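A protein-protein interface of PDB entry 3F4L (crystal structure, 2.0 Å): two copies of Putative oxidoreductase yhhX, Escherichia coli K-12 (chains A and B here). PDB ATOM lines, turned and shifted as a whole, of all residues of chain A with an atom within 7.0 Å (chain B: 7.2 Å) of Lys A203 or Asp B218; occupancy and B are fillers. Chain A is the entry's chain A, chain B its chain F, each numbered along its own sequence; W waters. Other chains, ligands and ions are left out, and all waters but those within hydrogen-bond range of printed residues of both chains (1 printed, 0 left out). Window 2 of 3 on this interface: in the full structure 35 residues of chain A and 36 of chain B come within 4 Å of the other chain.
No position is printed for both chains. Of the 9 pairs that touch across the chains among the printed residues, none has its exchanged pair printed and touching as well.
NE of Arg A198 is in hydrogen-bond range of O of Asp B218 (2.8 Å). The side-chain carboxylate (OD2) of Asp B218 lies within salt-bridge range of the side-chain amino group (NZ) of Lys A203, 2.5 Å away. The backbone carbonyl oxygen of Val B147 lies within hydrogen-bond range of the guanidinium group of Arg A198. The backbone carbonyl oxygen (O) of Leu A200 lies within hydrogen-bond range of the side-chain amino group (NZ) of Lys B241. NZ of Lys B220 lies within salt-bridge range of OD2 of Asp A196 (2.7 Å).
NZ of Lys B241 lies within salt-bridge range of OE2 of Glu B145 (3.3 Å). The backbone NH (N) of Arg A198 is in hydrogen-bond range of the backbone carbonyl oxygen (O) of Thr A209. N of Asp B191 lies within hydrogen-bond range of O of Phe B215 (2.8 Å). The backbone NH of Lys B220 lies within hydrogen-bond range of the backbone carbonyl oxygen of Val B147, at 3.2 Å. The guanidinium group of Arg A198 is in salt-bridge range of the side-chain carboxylate of Asp A196, 3.0 Å away. O of Ser A199 sits at hydrogen-bond distance from NZ of Lys A203, at 2.8 Å.
Asp A196 touches Phe B215. N of Lys B220 touches NH2 of Arg A198, 3.9 Å away. Val B147 touches Leu A200 (CB to CD1, 3.8 Å). Leu A200 touches Asp B218.
Of the printed residues of chain B, Lys A203 touches Asp B218 (2.5 Å). Of chain A, only Arg A198, Leu A200 and Lys A203 come within 4 Å of Asp B218. Of the printed residues of chain B, Leu A200 touches Val B147, Asp B218 and Lys B241. Printed residues of chain A within 4 Å of Lys B220: Asp A196 (2.7 Å) and Arg A198 (3.9 Å). Printed residues of chain B within 4 Å of Asp A196: Phe B215 (3.4 Å) and Lys B220 (2.7 Å). Printed residues of chain A within 4 Å of Phe B215: Asp A196 (3.4 Å). Printed residues of chain A within 4 Å of Lys B241: Leu A200 (3.4 Å). Glu B148 touches none of the printed residues of chain A. The nearest printed residue of chain B that does not touch Lys A203 is Glu B145 (6.0 Å). The nearest residue of chain A that does not touch Asp B218 is Ser A199 (4.5 Å). The nearest printed residue of chain B that does not touch Leu A200 is Leu B219 (5.4 Å).
Along chain B the printed residues that touch a printed residue of chain A span positions 147 to 241. Of the 12 printed residues of chain A, 4 touch a printed residue of chain B.
Water W1 bridges the backbone NH of Ser A199 (3.0 Å) and the side-chain carboxylate of Asp B218 (3.3 Å).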
ATOM      1  N   ASP A 196      20.251 -21.664  19.240  1.00  0.00           N
ATOM      2  CA  ASP A 196      20.070 -20.285  18.789  1.00  0.00           C
ATOM      3  C   ASP A 196      20.063 -20.436  17.268  1.00  0.00           C
ATOM      4  O   ASP A 196      21.114 -20.625  16.656  1.00  0.00           O
ATOM      5  CB  ASP A 196      21.240 -19.382  19.201  1.00  0.00           C
ATOM      6  CG  ASP A 196      21.290 -18.088  18.392  1.00  0.00           C
ATOM      7  OD1 ASP A 196      20.209 -17.524  18.099  1.00  0.00           O
ATOM      8  OD2 ASP A 196      22.406 -17.625  18.051  1.00  0.00           O
ATOM      9  N   ILE A 197      18.879 -20.371  16.670  1.00  0.00           N
ATOM     10  CA  ILE A 197      18.730 -20.536  15.230  1.00  0.00           C
ATOM     11  C   ILE A 197      17.963 -19.344  14.650  1.00  0.00           C
ATOM     12  O   ILE A 197      16.787 -19.141  14.963  1.00  0.00           O
ATOM     13  CB  ILE A 197      17.957 -21.840  14.919  1.00  0.00           C
ATOM     14  CG1 ILE A 197      18.642 -23.029  15.607  1.00  0.00           C
ATOM     15  CG2 ILE A 197      17.894 -22.066  13.404  1.00  0.00           C
ATOM     16  CD1 ILE A 197      17.849 -24.337  15.541  1.00  0.00           C
ATOM     17  N   ARG A 198      18.629 -18.569  13.796  1.00  0.00           N
ATOM     18  CA  ARG A 198      18.006 -17.387  13.216  1.00  0.00           C
ATOM     19  C   ARG A 198      18.160 -17.239  11.698  1.00  0.00           C
ATOM     20  O   ARG A 198      19.083 -17.784  11.088  1.00  0.00           O
ATOM     21  CB  ARG A 198      18.559 -16.130  13.899  1.00  0.00           C
ATOM     22  CG  ARG A 198      18.972 -16.361  15.336  1.00  0.00           C
ATOM     23  CD  ARG A 198      18.931 -15.094  16.189  1.00  0.00           C
ATOM     24  NE  ARG A 198      19.903 -14.061  15.832  1.00  0.00           N
ATOM     25  CZ  ARG A 198      21.226 -14.199  15.886  1.00  0.00           C
ATOM     26  NH1 ARG A 198      21.771 -15.344  16.273  1.00  0.00           N
ATOM     27  NH2 ARG A 198      22.011 -13.171  15.586  1.00  0.00           N
ATOM     28  N   SER A 199      17.231 -16.491  11.108  1.00  0.00           N
ATOM     29  CA  SER A 199      17.222 -16.200   9.677  1.00  0.00           C
ATOM     30  C   SER A 199      17.434 -14.688   9.601  1.00  0.00           C
ATOM     31  O   SER A 199      16.505 -13.911   9.827  1.00  0.00           O
ATOM     32  CB  SER A 199      15.869 -16.586   9.073  1.00  0.00           C
ATOM     33  OG  SER A 199      15.848 -16.299   7.688  1.00  0.00           O
ATOM     34  N   LEU A 200      18.661 -14.278   9.296  1.00  0.00           N
ATOM     35  CA  LEU A 200      19.023 -12.862   9.261  1.00  0.00           C
ATOM     36  C   LEU A 200      19.012 -12.128   7.924  1.00  0.00           C
ATOM     37  O   LEU A 200      18.556 -10.993   7.845  1.00  0.00           O
ATOM     38  CB  LEU A 200      20.415 -12.688   9.875  1.00  0.00           C
ATOM     39  CG  LEU A 200      20.607 -13.076  11.342  1.00  0.00           C
ATOM     40  CD1 LEU A 200      22.092 -12.988  11.688  1.00  0.00           C
ATOM     41  CD2 LEU A 200      19.795 -12.162  12.237  1.00  0.00           C
ATOM     42  N   ARG A 201      19.553 -12.754   6.885  1.00  0.00           N
ATOM     43  CA  ARG A 201      19.633 -12.115   5.578  1.00  0.00           C
ATOM     44  C   ARG A 201      18.295 -11.871   4.894  1.00  0.00           C
ATOM     45  O   ARG A 201      18.056 -10.787   4.356  1.00  0.00           O
ATOM     46  CB  ARG A 201      20.532 -12.938   4.661  1.00  0.00           C
ATOM     47  CG  ARG A 201      21.979 -12.993   5.108  1.00  0.00           C
ATOM     48  CD  ARG A 201      22.784 -13.865   4.173  1.00  0.00           C
ATOM     49  NE  ARG A 201      22.242 -15.216   4.122  1.00  0.00           N
ATOM     50  CZ  ARG A 201      22.661 -16.161   3.286  1.00  0.00           C
ATOM     51  NH1 ARG A 201      23.632 -15.905   2.421  1.00  0.00           N
ATOM     52  NH2 ARG A 201      22.111 -17.368   3.323  1.00  0.00           N
ATOM     53  N   ASN A 202      17.434 -12.879   4.896  1.00  0.00           N
ATOM     54  CA  ASN A 202      16.121 -12.753   4.270  1.00  0.00           C
ATOM     55  C   ASN A 202      15.107 -13.484   5.126  1.00  0.00           C
ATOM     56  O   ASN A 202      15.092 -14.715   5.157  1.00  0.00           O
ATOM     57  CB  ASN A 202      16.129 -13.362   2.868  1.00  0.00           C
ATOM     58  CG  ASN A 202      14.852 -13.069   2.108  1.00  0.00           C
ATOM     59  OD1 ASN A 202      13.780 -12.972   2.704  1.00  0.00           O
ATOM     60  ND2 ASN A 202      14.956 -12.940   0.784  1.00  0.00           N
ATOM     61  N   LYS A 203      14.258 -12.727   5.813  1.00  0.00           N
ATOM     62  CA  LYS A 203      13.260 -13.319   6.699  1.00  0.00           C
ATOM     63  C   LYS A 203      12.309 -14.315   6.043  1.00  0.00           C
ATOM     64  O   LYS A 203      11.580 -15.026   6.732  1.00  0.00           O
ATOM     65  CB  LYS A 203      12.457 -12.218   7.401  1.00  0.00           C
ATOM     66  CG  LYS A 203      13.161 -11.613   8.609  1.00  0.00           C
ATOM     67  CD  LYS A 203      13.455 -12.680   9.650  1.00  0.00           C
ATOM     68  CE  LYS A 203      14.087 -12.100  10.907  1.00  0.00           C
ATOM     69  NZ  LYS A 203      15.410 -11.457  10.662  1.00  0.00           N
ATOM     70  N   ALA A 204      12.316 -14.385   4.716  1.00  0.00           N
ATOM     71  CA  ALA A 204      11.436 -15.321   4.036  1.00  0.00           C
ATOM     72  C   ALA A 204      12.074 -16.706   3.951  1.00  0.00           C
ATOM     73  O   ALA A 204      11.379 -17.698   3.743  1.00  0.00           O
ATOM     74  CB  ALA A 204      11.110 -14.807   2.629  1.00  0.00           C
ATOM     75  N   ASN A 205      13.395 -16.763   4.121  1.00  0.00           N
ATOM     76  CA  ASN A 205      14.157 -18.012   4.022  1.00  0.00           C
ATOM     77  C   ASN A 205      14.375 -18.795   5.321  1.00  0.00           C
ATOM     78  O   ASN A 205      14.172 -18.280   6.422  1.00  0.00           O
ATOM     79  CB  ASN A 205      15.541 -17.724   3.419  1.00  0.00           C
ATOM     80  CG  ASN A 205      15.462 -17.128   2.031  1.00  0.00           C
ATOM     81  OD1 ASN A 205      14.377 -16.901   1.506  1.00  0.00           O
ATOM     82  ND2 ASN A 205      16.615 -16.872   1.432  1.00  0.00           N
ATOM     83  N   PRO A 206      14.785 -20.069   5.199  1.00  0.00           N
ATOM     84  CA  PRO A 206      15.044 -20.904   6.376  1.00  0.00           C
ATOM     85  C   PRO A 206      16.273 -20.293   7.076  1.00  0.00           C
ATOM     86  O   PRO A 206      16.927 -19.411   6.522  1.00  0.00           O
ATOM     87  CB  PRO A 206      15.351 -22.269   5.764  1.00  0.00           C
ATOM     88  CG  PRO A 206      14.507 -22.267   4.505  1.00  0.00           C
ATOM     89  CD  PRO A 206      14.775 -20.883   3.969  1.00  0.00           C
ATOM     90  N   THR A 209      21.764 -18.823  10.175  1.00  0.00           N
ATOM     91  CA  THR A 209      22.609 -18.506  11.314  1.00  0.00           C
ATOM     92  C   THR A 209      22.256 -19.436  12.467  1.00  0.00           C
ATOM     93  O   THR A 209      21.078 -19.627  12.767  1.00  0.00           O
ATOM     94  CB  THR A 209      22.344 -17.065  11.775  1.00  0.00           C
ATOM     95  OG1 THR A 209      22.405 -16.191  10.642  1.00  0.00           O
ATOM     96  CG2 THR A 209      23.363 -16.632  12.827  1.00  0.00           C
ATOM     97  N   GLU B 145      23.375  -2.950   9.838  1.00  0.00           N
ATOM     98  CA  GLU B 145      22.532  -3.467  10.921  1.00  0.00           C
ATOM     99  C   GLU B 145      23.339  -4.450  11.767  1.00  0.00           C
ATOM    100  O   GLU B 145      23.904  -5.409  11.237  1.00  0.00           O
ATOM    101  CB  GLU B 145      21.293  -4.171  10.347  1.00  0.00           C
ATOM    102  CG  GLU B 145      20.362  -4.757  11.415  1.00  0.00           C
ATOM    103  CD  GLU B 145      19.104  -5.401  10.838  1.00  0.00           C
ATOM    104  OE1 GLU B 145      18.350  -4.711  10.120  1.00  0.00           O
ATOM    105  OE2 GLU B 145      18.865  -6.601  11.109  1.00  0.00           O
ATOM    106  N   ILE B 146      23.383  -4.219  13.077  1.00  0.00           N
ATOM    107  CA  ILE B 146      24.156  -5.074  13.977  1.00  0.00           C
ATOM    108  C   ILE B 146      23.454  -6.398  14.282  1.00  0.00           C
ATOM    109  O   ILE B 146      22.316  -6.411  14.756  1.00  0.00           O
ATOM    110  CB  ILE B 146      24.445  -4.352  15.310  1.00  0.00           C
ATOM    111  CG1 ILE B 146      25.099  -2.984  15.045  1.00  0.00           C
ATOM    112  CG2 ILE B 146      25.333  -5.233  16.191  1.00  0.00           C
ATOM    113  CD1 ILE B 146      26.385  -3.046  14.262  1.00  0.00           C
ATOM    114  N   VAL B 147      24.133  -7.509  14.024  1.00  0.00           N
ATOM    115  CA  VAL B 147      23.532  -8.811  14.279  1.00  0.00           C
ATOM    116  C   VAL B 147      24.194  -9.606  15.416  1.00  0.00           C
ATOM    117  O   VAL B 147      23.603 -10.549  15.950  1.00  0.00           O
ATOM    118  CB  VAL B 147      23.514  -9.664  13.000  1.00  0.00           C
ATOM    119  CG1 VAL B 147      22.691  -8.947  11.919  1.00  0.00           C
ATOM    120  CG2 VAL B 147      24.932  -9.922  12.519  1.00  0.00           C
ATOM    121  N   GLU B 148      25.418  -9.240  15.785  1.00  0.00           N
ATOM    122  CA  GLU B 148      26.078  -9.940  16.879  1.00  0.00           C
ATOM    123  C   GLU B 148      27.186  -9.123  17.547  1.00  0.00           C
ATOM    124  O   GLU B 148      27.961  -8.412  16.891  1.00  0.00           O
ATOM    125  CB  GLU B 148      26.622 -11.309  16.406  1.00  0.00           C
ATOM    126  CG  GLU B 148      26.956 -12.273  17.573  1.00  0.00           C
ATOM    127  CD  GLU B 148      26.938 -13.753  17.184  1.00  0.00           C
ATOM    128  OE1 GLU B 148      25.938 -14.214  16.582  1.00  0.00           O
ATOM    129  OE2 GLU B 148      27.919 -14.464  17.494  1.00  0.00           O
ATOM    130  N   ASP B 191      14.836  -9.462  24.882  1.00  0.00           N
ATOM    131  CA  ASP B 191      13.608 -10.257  24.835  1.00  0.00           C
ATOM    132  C   ASP B 191      13.812 -11.592  25.542  1.00  0.00           C
ATOM    133  O   ASP B 191      12.921 -12.076  26.254  1.00  0.00           O
ATOM    134  CB  ASP B 191      13.187 -10.543  23.386  1.00  0.00           C
ATOM    135  CG  ASP B 191      12.986  -9.280  22.566  1.00  0.00           C
ATOM    136  OD1 ASP B 191      12.339  -8.338  23.064  1.00  0.00           O
ATOM    137  OD2 ASP B 191      13.466  -9.239  21.409  1.00  0.00           O
ATOM    138  N   PHE B 215      19.194 -11.661  23.772  1.00  0.00           N
ATOM    139  CA  PHE B 215      18.566 -11.571  22.453  1.00  0.00           C
ATOM    140  C   PHE B 215      17.684 -10.348  22.278  1.00  0.00           C
ATOM    141  O   PHE B 215      16.704 -10.182  22.987  1.00  0.00           O
ATOM    142  CB  PHE B 215      17.725 -12.819  22.178  1.00  0.00           C
ATOM    143  CG  PHE B 215      18.513 -14.092  22.195  1.00  0.00           C
ATOM    144  CD1 PHE B 215      18.970 -14.628  23.397  1.00  0.00           C
ATOM    145  CD2 PHE B 215      18.827 -14.743  21.003  1.00  0.00           C
ATOM    146  CE1 PHE B 215      19.733 -15.798  23.416  1.00  0.00           C
ATOM    147  CE2 PHE B 215      19.597 -15.921  21.012  1.00  0.00           C
ATOM    148  CZ  PHE B 215      20.046 -16.444  22.214  1.00  0.00           C
ATOM    149  N   TYR B 216      18.046  -9.494  21.329  1.00  0.00           N
ATOM    150  CA  TYR B 216      17.280  -8.293  21.032  1.00  0.00           C
ATOM    151  C   TYR B 216      16.747  -8.461  19.624  1.00  0.00           C
ATOM    152  O   TYR B 216      17.380  -8.029  18.651  1.00  0.00           O
ATOM    153  CB  TYR B 216      18.164  -7.049  21.088  1.00  0.00           C
ATOM    154  CG  TYR B 216      18.768  -6.773  22.440  1.00  0.00           C
ATOM    155  CD1 TYR B 216      19.938  -7.418  22.856  1.00  0.00           C
ATOM    156  CD2 TYR B 216      18.189  -5.837  23.299  1.00  0.00           C
ATOM    157  CE1 TYR B 216      20.517  -7.129  24.082  1.00  0.00           C
ATOM    158  CE2 TYR B 216      18.760  -5.543  24.530  1.00  0.00           C
ATOM    159  CZ  TYR B 216      19.925  -6.188  24.914  1.00  0.00           C
ATOM    160  OH  TYR B 216      20.503  -5.865  26.119  1.00  0.00           O
ATOM    161  N   GLY B 217      15.584  -9.089  19.512  1.00  0.00           N
ATOM    162  CA  GLY B 217      15.023  -9.318  18.196  1.00  0.00           C
ATOM    163  C   GLY B 217      15.910 -10.341  17.517  1.00  0.00           C
ATOM    164  O   GLY B 217      15.967 -11.495  17.949  1.00  0.00           O
ATOM    165  N   ASP B 218      16.614  -9.924  16.468  1.00  0.00           N
ATOM    166  CA  ASP B 218      17.514 -10.825  15.755  1.00  0.00           C
ATOM    167  C   ASP B 218      18.974 -10.605  16.110  1.00  0.00           C
ATOM    168  O   ASP B 218      19.852 -11.299  15.599  1.00  0.00           O
ATOM    169  CB  ASP B 218      17.342 -10.679  14.242  1.00  0.00           C
ATOM    170  CG  ASP B 218      16.074 -11.328  13.744  1.00  0.00           C
ATOM    171  OD1 ASP B 218      15.855 -12.519  14.063  1.00  0.00           O
ATOM    172  OD2 ASP B 218      15.300 -10.652  13.038  1.00  0.00           O
ATOM    173  N   LEU B 219      19.233  -9.623  16.963  1.00  0.00           N
ATOM    174  CA  LEU B 219      20.595  -9.327  17.387  1.00  0.00           C
ATOM    175  C   LEU B 219      20.883 -10.137  18.645  1.00  0.00           C
ATOM    176  O   LEU B 219      20.062 -10.182  19.556  1.00  0.00           O
ATOM    177  CB  LEU B 219      20.744  -7.825  17.675  1.00  0.00           C
ATOM    178  CG  LEU B 219      21.882  -7.314  18.564  1.00  0.00           C
ATOM    179  CD1 LEU B 219      23.222  -7.796  18.060  1.00  0.00           C
ATOM    180  CD2 LEU B 219      21.852  -5.797  18.581  1.00  0.00           C
ATOM    181  N   LYS B 220      22.030 -10.801  18.679  1.00  0.00           N
ATOM    182  CA  LYS B 220      22.413 -11.570  19.856  1.00  0.00           C
ATOM    183  C   LYS B 220      23.679 -10.968  20.459  1.00  0.00           C
ATOM    184  O   LYS B 220      24.699 -10.844  19.780  1.00  0.00           O
ATOM    185  CB  LYS B 220      22.674 -13.040  19.515  1.00  0.00           C
ATOM    186  CG  LYS B 220      23.109 -13.826  20.738  1.00  0.00           C
ATOM    187  CD  LYS B 220      23.284 -15.309  20.488  1.00  0.00           C
ATOM    188  CE  LYS B 220      24.475 -15.596  19.596  1.00  0.00           C
ATOM    189  NZ  LYS B 220      24.645 -17.074  19.459  1.00  0.00           N
ATOM    190  N   LYS B 241      25.615  -6.425   9.166  1.00  0.00           N
ATOM    191  CA  LYS B 241      25.374  -6.875   7.802  1.00  0.00           C
ATOM    192  C   LYS B 241      26.365  -6.356   6.772  1.00  0.00           C
ATOM    193  O   LYS B 241      26.534  -6.968   5.714  1.00  0.00           O
ATOM    194  CB  LYS B 241      23.954  -6.503   7.376  1.00  0.00           C
ATOM    195  CG  LYS B 241      22.903  -7.310   8.098  1.00  0.00           C
ATOM    196  CD  LYS B 241      21.504  -6.982   7.621  1.00  0.00           C
ATOM    197  CE  LYS B 241      20.520  -7.966   8.239  1.00  0.00           C
ATOM    198  NZ  LYS B 241      19.116  -7.596   7.949  1.00  0.00           N
HETATM  199  O   HOH W   1      15.134 -15.524  12.999  1.00  0.00           O
